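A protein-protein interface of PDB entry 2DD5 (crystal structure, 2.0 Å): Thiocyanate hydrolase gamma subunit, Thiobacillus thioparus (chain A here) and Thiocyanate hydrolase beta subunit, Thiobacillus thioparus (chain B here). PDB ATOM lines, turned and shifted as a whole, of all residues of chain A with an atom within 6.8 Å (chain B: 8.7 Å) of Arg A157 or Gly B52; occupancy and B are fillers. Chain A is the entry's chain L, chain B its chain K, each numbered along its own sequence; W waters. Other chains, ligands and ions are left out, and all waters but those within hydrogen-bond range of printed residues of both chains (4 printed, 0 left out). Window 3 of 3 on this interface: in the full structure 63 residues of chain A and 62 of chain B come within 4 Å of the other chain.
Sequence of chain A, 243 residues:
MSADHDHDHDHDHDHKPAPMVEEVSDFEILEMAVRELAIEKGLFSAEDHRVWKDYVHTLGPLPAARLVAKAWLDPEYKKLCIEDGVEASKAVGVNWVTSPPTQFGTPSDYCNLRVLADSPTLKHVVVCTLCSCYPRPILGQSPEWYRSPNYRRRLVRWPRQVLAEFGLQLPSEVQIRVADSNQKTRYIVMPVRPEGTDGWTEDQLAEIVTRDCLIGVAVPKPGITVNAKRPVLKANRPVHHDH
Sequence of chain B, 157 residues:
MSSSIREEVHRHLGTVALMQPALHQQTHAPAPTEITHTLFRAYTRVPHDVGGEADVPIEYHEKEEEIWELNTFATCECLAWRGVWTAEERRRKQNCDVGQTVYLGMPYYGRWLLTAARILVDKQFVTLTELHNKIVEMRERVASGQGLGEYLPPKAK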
ATOM      1  N   THR A 129      30.822 -21.518  -1.013  1.00  0.00           N
ATOM      2  CA  THR A 129      29.572 -22.239  -0.800  1.00  0.00           C
ATOM      3  C   THR A 129      29.527 -23.545  -1.575  1.00  0.00           C
ATOM      4  O   THR A 129      28.833 -24.474  -1.175  1.00  0.00           O
ATOM      5  CB  THR A 129      28.337 -21.380  -1.173  1.00  0.00           C
ATOM      6  OG1 THR A 129      28.355 -21.087  -2.574  1.00  0.00           O
ATOM      7  CG2 THR A 129      28.331 -20.070  -0.375  1.00  0.00           C
ATOM      8  N   ARG A 152      28.708 -23.154   4.851  1.00  0.00           N
ATOM      9  CA  ARG A 152      28.491 -22.908   3.428  1.00  0.00           C
ATOM     10  C   ARG A 152      27.045 -22.540   3.090  1.00  0.00           C
ATOM     11  O   ARG A 152      26.783 -21.874   2.092  1.00  0.00           O
ATOM     12  CB  ARG A 152      28.936 -24.133   2.622  1.00  0.00           C
ATOM     13  CG  ARG A 152      30.458 -24.381   2.689  1.00  0.00           C
ATOM     14  CD  ARG A 152      30.802 -25.767   2.154  1.00  0.00           C
ATOM     15  NE  ARG A 152      30.120 -25.988   0.889  1.00  0.00           N
ATOM     16  CZ  ARG A 152      29.672 -27.166   0.471  1.00  0.00           C
ATOM     17  NH1 ARG A 152      29.052 -27.254  -0.700  1.00  0.00           N
ATOM     18  NH2 ARG A 152      29.844 -28.251   1.217  1.00  0.00           N
ATOM     19  N   ARG A 153      26.101 -22.980   3.909  1.00  0.00           N
ATOM     20  CA  ARG A 153      24.696 -22.645   3.664  1.00  0.00           C
ATOM     21  C   ARG A 153      24.317 -21.282   4.254  1.00  0.00           C
ATOM     22  O   ARG A 153      23.611 -20.488   3.630  1.00  0.00           O
ATOM     23  CB  ARG A 153      23.773 -23.680   4.316  1.00  0.00           C
ATOM     24  CG  ARG A 153      23.691 -25.034   3.627  1.00  0.00           C
ATOM     25  CD  ARG A 153      22.922 -26.015   4.515  1.00  0.00           C
ATOM     26  NE  ARG A 153      22.690 -27.283   3.834  1.00  0.00           N
ATOM     27  CZ  ARG A 153      22.723 -28.471   4.429  1.00  0.00           C
ATOM     28  NH1 ARG A 153      22.982 -28.564   5.727  1.00  0.00           N
ATOM     29  NH2 ARG A 153      22.502 -29.568   3.720  1.00  0.00           N
ATOM     30  N   ARG A 154      24.797 -21.026   5.464  1.00  0.00           N
ATOM     31  CA  ARG A 154      24.421 -19.822   6.199  1.00  0.00           C
ATOM     32  C   ARG A 154      25.124 -18.487   6.011  1.00  0.00           C
ATOM     33  O   ARG A 154      24.468 -17.444   6.012  1.00  0.00           O
ATOM     34  CB  ARG A 154      24.427 -20.136   7.699  1.00  0.00           C
ATOM     35  CG  ARG A 154      23.481 -21.260   8.118  1.00  0.00           C
ATOM     36  CD  ARG A 154      23.251 -21.219   9.619  1.00  0.00           C
ATOM     37  NE  ARG A 154      24.483 -21.404  10.378  1.00  0.00           N
ATOM     38  CZ  ARG A 154      24.713 -20.866  11.573  1.00  0.00           C
ATOM     39  NH1 ARG A 154      23.796 -20.099  12.154  1.00  0.00           N
ATOM     40  NH2 ARG A 154      25.869 -21.090  12.187  1.00  0.00           N
ATOM     41  N   LEU A 155      26.442 -18.496   5.876  1.00  0.00           N
ATOM     42  CA  LEU A 155      27.166 -17.229   5.770  1.00  0.00           C
ATOM     43  C   LEU A 155      26.669 -16.254   4.712  1.00  0.00           C
ATOM     44  O   LEU A 155      26.516 -15.060   4.991  1.00  0.00           O
ATOM     45  CB  LEU A 155      28.665 -17.472   5.563  1.00  0.00           C
ATOM     46  CG  LEU A 155      29.530 -16.208   5.709  1.00  0.00           C
ATOM     47  CD1 LEU A 155      29.641 -15.824   7.187  1.00  0.00           C
ATOM     48  CD2 LEU A 155      30.909 -16.456   5.125  1.00  0.00           C
ATOM     49  N   VAL A 156      26.405 -16.742   3.504  1.00  0.00           N
ATOM     50  CA  VAL A 156      25.965 -15.850   2.443  1.00  0.00           C
ATOM     51  C   VAL A 156      24.604 -15.211   2.674  1.00  0.00           C
ATOM     52  O   VAL A 156      24.325 -14.143   2.128  1.00  0.00           O
ATOM     53  CB  VAL A 156      25.939 -16.559   1.057  1.00  0.00           C
ATOM     54  CG1 VAL A 156      27.349 -17.004   0.677  1.00  0.00           C
ATOM     55  CG2 VAL A 156      24.966 -17.745   1.077  1.00  0.00           C
ATOM     56  N   ARG A 157      23.770 -15.843   3.495  1.00  0.00           N
ATOM     57  CA  ARG A 157      22.425 -15.328   3.733  1.00  0.00           C
ATOM     58  C   ARG A 157      22.207 -14.630   5.068  1.00  0.00           C
ATOM     59  O   ARG A 157      21.415 -13.691   5.154  1.00  0.00           O
ATOM     60  CB  ARG A 157      21.404 -16.465   3.584  1.00  0.00           C
ATOM     61  CG  ARG A 157      19.951 -16.018   3.666  1.00  0.00           C
ATOM     62  CD  ARG A 157      19.007 -17.135   3.203  1.00  0.00           C
ATOM     63  NE  ARG A 157      17.657 -16.628   2.962  1.00  0.00           N
ATOM     64  CZ  ARG A 157      16.723 -17.273   2.267  1.00  0.00           C
ATOM     65  NH1 ARG A 157      16.984 -18.466   1.742  1.00  0.00           N
ATOM     66  NH2 ARG A 157      15.533 -16.709   2.074  1.00  0.00           N
ATOM     67  N   TRP A 158      22.890 -15.096   6.105  1.00  0.00           N
ATOM     68  CA  TRP A 158      22.762 -14.513   7.441  1.00  0.00           C
ATOM     69  C   TRP A 158      24.158 -14.213   7.986  1.00  0.00           C
ATOM     70  O   TRP A 158      24.503 -14.628   9.091  1.00  0.00           O
ATOM     71  CB  TRP A 158      22.051 -15.503   8.369  1.00  0.00           C
ATOM     72  CG  TRP A 158      20.671 -15.884   7.912  1.00  0.00           C
ATOM     73  CD1 TRP A 158      19.529 -15.136   8.027  1.00  0.00           C
ATOM     74  CD2 TRP A 158      20.287 -17.107   7.268  1.00  0.00           C
ATOM     75  NE1 TRP A 158      18.458 -15.824   7.495  1.00  0.00           N
ATOM     76  CE2 TRP A 158      18.897 -17.034   7.023  1.00  0.00           C
ATOM     77  CE3 TRP A 158      20.984 -18.258   6.876  1.00  0.00           C
ATOM     78  CZ2 TRP A 158      18.187 -18.072   6.401  1.00  0.00           C
ATOM     79  CZ3 TRP A 158      20.277 -19.294   6.255  1.00  0.00           C
ATOM     80  CH2 TRP A 158      18.893 -19.190   6.027  1.00  0.00           C
ATOM     81  N   PRO A 159      24.971 -13.466   7.226  1.00  0.00           N
ATOM     82  CA  PRO A 159      26.327 -13.161   7.699  1.00  0.00           C
ATOM     83  C   PRO A 159      26.413 -12.522   9.079  1.00  0.00           C
ATOM     84  O   PRO A 159      27.261 -12.902   9.884  1.00  0.00           O
ATOM     85  CB  PRO A 159      26.895 -12.277   6.585  1.00  0.00           C
ATOM     86  CG  PRO A 159      25.670 -11.631   5.990  1.00  0.00           C
ATOM     87  CD  PRO A 159      24.675 -12.762   5.966  1.00  0.00           C
ATOM     88  N   ARG A 160      25.526 -11.568   9.355  1.00  0.00           N
ATOM     89  CA  ARG A 160      25.509 -10.880  10.647  1.00  0.00           C
ATOM     90  C   ARG A 160      25.294 -11.859  11.786  1.00  0.00           C
ATOM     91  O   ARG A 160      25.937 -11.769  12.835  1.00  0.00           O
ATOM     92  CB  ARG A 160      24.381  -9.845  10.685  1.00  0.00           C
ATOM     93  CG  ARG A 160      24.514  -8.739   9.659  1.00  0.00           C
ATOM     94  CD  ARG A 160      25.255  -7.566  10.233  1.00  0.00           C
ATOM     95  NE  ARG A 160      25.437  -6.499   9.254  1.00  0.00           N
ATOM     96  CZ  ARG A 160      25.967  -5.317   9.549  1.00  0.00           C
ATOM     97  NH1 ARG A 160      26.354  -5.065  10.791  1.00  0.00           N
ATOM     98  NH2 ARG A 160      26.118  -4.394   8.608  1.00  0.00           N
ATOM     99  N   GLN A 161      24.373 -12.791  11.581  1.00  0.00           N
ATOM    100  CA  GLN A 161      24.070 -13.769  12.609  1.00  0.00           C
ATOM    101  C   GLN A 161      25.224 -14.749  12.795  1.00  0.00           C
ATOM    102  O   GLN A 161      25.596 -15.064  13.924  1.00  0.00           O
ATOM    103  CB  GLN A 161      22.766 -14.502  12.263  1.00  0.00           C
ATOM    104  CG  GLN A 161      21.536 -13.579  12.276  1.00  0.00           C
ATOM    105  CD  GLN A 161      21.350 -12.792  10.983  1.00  0.00           C
ATOM    106  OE1 GLN A 161      22.254 -12.706  10.153  1.00  0.00           O
ATOM    107  NE2 GLN A 161      20.169 -12.206  10.815  1.00  0.00           N
ATOM    108  N   VAL A 178      30.166 -10.396   1.840  1.00  0.00           N
ATOM    109  CA  VAL A 178      30.532 -11.802   1.845  1.00  0.00           C
ATOM    110  C   VAL A 178      31.097 -12.100   0.461  1.00  0.00           C
ATOM    111  O   VAL A 178      30.502 -11.731  -0.552  1.00  0.00           O
ATOM    112  CB  VAL A 178      29.308 -12.721   2.082  1.00  0.00           C
ATOM    113  CG1 VAL A 178      29.744 -14.185   2.031  1.00  0.00           C
ATOM    114  CG2 VAL A 178      28.663 -12.405   3.432  1.00  0.00           C
ATOM    115  N   ASP B  49      25.663 -27.106  -4.567  1.00  0.00           N
ATOM    116  CA  ASP B  49      25.088 -25.759  -4.514  1.00  0.00           C
ATOM    117  C   ASP B  49      24.146 -25.597  -3.319  1.00  0.00           C
ATOM    118  O   ASP B  49      22.925 -25.665  -3.471  1.00  0.00           O
ATOM    119  CB  ASP B  49      24.343 -25.496  -5.821  1.00  0.00           C
ATOM    120  CG  ASP B  49      23.934 -24.050  -5.983  1.00  0.00           C
ATOM    121  OD1 ASP B  49      24.340 -23.207  -5.156  1.00  0.00           O
ATOM    122  OD2 ASP B  49      23.212 -23.762  -6.956  1.00  0.00           O
ATOM    123  N   VAL B  50      24.713 -25.357  -2.141  1.00  0.00           N
ATOM    124  CA  VAL B  50      23.913 -25.241  -0.923  1.00  0.00           C
ATOM    125  C   VAL B  50      23.706 -23.832  -0.346  1.00  0.00           C
ATOM    126  O   VAL B  50      22.950 -23.661   0.608  1.00  0.00           O
ATOM    127  CB  VAL B  50      24.514 -26.136   0.185  1.00  0.00           C
ATOM    128  CG1 VAL B  50      24.696 -27.578  -0.346  1.00  0.00           C
ATOM    129  CG2 VAL B  50      25.857 -25.568   0.648  1.00  0.00           C
ATOM    130  N   GLY B  51      24.365 -22.832  -0.925  1.00  0.00           N
ATOM    131  CA  GLY B  51      24.237 -21.471  -0.418  1.00  0.00           C
ATOM    132  C   GLY B  51      22.807 -20.966  -0.289  1.00  0.00           C
ATOM    133  O   GLY B  51      22.041 -21.008  -1.245  1.00  0.00           O
ATOM    134  N   GLY B  52      22.443 -20.492   0.900  1.00  0.00           N
ATOM    135  CA  GLY B  52      21.098 -19.979   1.099  1.00  0.00           C
ATOM    136  C   GLY B  52      20.120 -20.954   1.732  1.00  0.00           C
ATOM    137  O   GLY B  52      19.024 -20.554   2.131  1.00  0.00           O
ATOM    138  N   GLU B  53      20.494 -22.228   1.827  1.00  0.00           N
ATOM    139  CA  GLU B  53      19.607 -23.217   2.433  1.00  0.00           C
ATOM    140  C   GLU B  53      19.543 -22.972   3.933  1.00  0.00           C
ATOM    141  O   GLU B  53      20.548 -22.656   4.561  1.00  0.00           O
ATOM    142  CB  GLU B  53      20.114 -24.638   2.167  1.00  0.00           C
ATOM    143  CG  GLU B  53      20.047 -25.068   0.708  1.00  0.00           C
ATOM    144  CD  GLU B  53      20.686 -26.432   0.471  1.00  0.00           C
ATOM    145  OE1 GLU B  53      21.052 -27.106   1.456  1.00  0.00           O
ATOM    146  OE2 GLU B  53      20.817 -26.830  -0.706  1.00  0.00           O
ATOM    147  N   ALA B  54      18.358 -23.114   4.511  1.00  0.00           N
ATOM    148  CA  ALA B  54      18.204 -22.905   5.943  1.00  0.00           C
ATOM    149  C   ALA B  54      18.944 -23.982   6.731  1.00  0.00           C
ATOM    150  O   ALA B  54      18.909 -25.156   6.372  1.00  0.00           O
ATOM    151  CB  ALA B  54      16.724 -22.921   6.313  1.00  0.00           C
ATOM    152  N   ASP B  55      19.642 -23.577   7.786  1.00  0.00           N
ATOM    153  CA  ASP B  55      20.340 -24.531   8.642  1.00  0.00           C
ATOM    154  C   ASP B  55      20.368 -23.922  10.034  1.00  0.00           C
ATOM    155  O   ASP B  55      20.125 -22.723  10.199  1.00  0.00           O
ATOM    156  CB  ASP B  55      21.768 -24.805   8.152  1.00  0.00           C
ATOM    157  CG  ASP B  55      22.295 -26.165   8.621  1.00  0.00           C
ATOM    158  OD1 ASP B  55      21.838 -26.667   9.675  1.00  0.00           O
ATOM    159  OD2 ASP B  55      23.176 -26.733   7.945  1.00  0.00           O
HETATM  160  O   HOH W   1      26.018 -22.483  -3.155  1.00  0.00           O
HETATM  161  O   HOH W   2      20.025 -27.626   6.905  1.00  0.00           O
HETATM  162  O   HOH W   3      20.867 -20.528  11.817  1.00  0.00           O
HETATM  163  O   HOH W   4      21.694 -29.623   0.830  1.00  0.00           O
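The backbone NH (N) of Gly B52 is in hydrogen-bond range of the backbone carbonyl oxygen (O) of Arg A153 (3.0 Å). The guanidinium group (NH1) of Arg A157 sits at hydrogen-bond distance from the backbone carbonyl oxygen (O) of Gly B52 (2.9 Å). The side-chain carboxylate (OE1) of Glu B53 lies within salt-bridge range of the guanidinium group (NE) of Arg A153, 2.9 Å away. The guanidinium group (NH1) of Arg A153 is in salt-bridge range of the side-chain carboxylate (OD2) of Asp B55, at 2.9 Å.
Water W4 lies within hydrogen-bond range of the side-chain carboxylate of Glu B53 (2.7 Å) and the guanidinium group of Arg A153 (3.0 Å). Water W1 lies within hydrogen-bond range of the side-chain carboxylate (OD1) of Asp B49 (2.7 Å), the side-chain hydroxyl (OG1) of Thr A129 (2.8 Å), the backbone NH (N) of Gly B51 (2.8 Å) and the backbone NH (N) of Val B50 (3.3 Å). Water W2 lies within hydrogen-bond range of the backbone carbonyl oxygen (O) of Ala B54 (2.8 Å), the guanidinium group (NH1) of Arg A153 (3.3 Å) and the side-chain carboxylate (OD2) of Asp B55 (3.4 Å). Water W3 bridges the backbone carbonyl oxygen (O) of Asp B55 (2.8 Å) and the guanidinium group (NH1) of Arg A154 (3.0 Å).
Of chain B, only Gly B52 (2.9 Å) comes within 4 Å of Arg A157. Gly B52 touches just these residues of chain A: Arg A153 (3.0 Å), Val A156 (3.7 Å) and Arg A157 (2.9 Å). Trp A158 touches just these residues of chain B: Glu B53 (3.8 Å) and Ala B54 (3.8 Å). Of the printed residues of chain B, Val A156 touches Gly B52 (3.7 Å). Printed residues of chain A within 4 Å of Val B50: Thr A129 (3.7 Å), Arg A152 (3.9 Å) and Arg A153 (3.4 Å). Of the printed residues of chain A, Ala B54 touches Trp A158. Printed residues of chain B within 4 Å of Arg A153: Val B50, Gly B52, Glu B53 and Asp B55. The nearest residue of chain A that does not touch Gly B52 is Trp A158 (4.1 Å).
Val B50 touches Thr A129 (CG2 to O, 3.7 Å). NH1 of Arg A152 touches CG2 of Val B50, 3.9 Å away. Gly B51 touches Arg A152 (CA to O, 3.6 Å). Val B50 touches Arg A153. Asp B55 touches Arg A154 (O to CD, 3.5 Å). Val A156 touches Gly B52. Trp A158 touches Glu B53. Ala B54 touches Trp A158 (CA to CH2, 3.8 Å).
The backbone carbonyl oxygen of Thr A129 sits at hydrogen-bond distance from the guanidinium group of Arg A152. The side-chain amide oxygen of Gln A161 lies close to the backbone carbonyl oxygen of Trp A158 (3.1 Å).
Hydrophobic or aromatic side chains of chain B within 4 Å of the printed part of chain A: Val B50. Hydrophobic or aromatic side chains of chain A within 4 Å of the printed part of chain B: Val A156 and Trp A158. Among the printed residues, Asp or Glu carboxylates within 4 Å of a Lys or Arg side-chain nitrogen of the other chain: Arg A153 with Glu B53 (2.9 Å) and Arg A153 with Asp B55 (2.9 Å).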
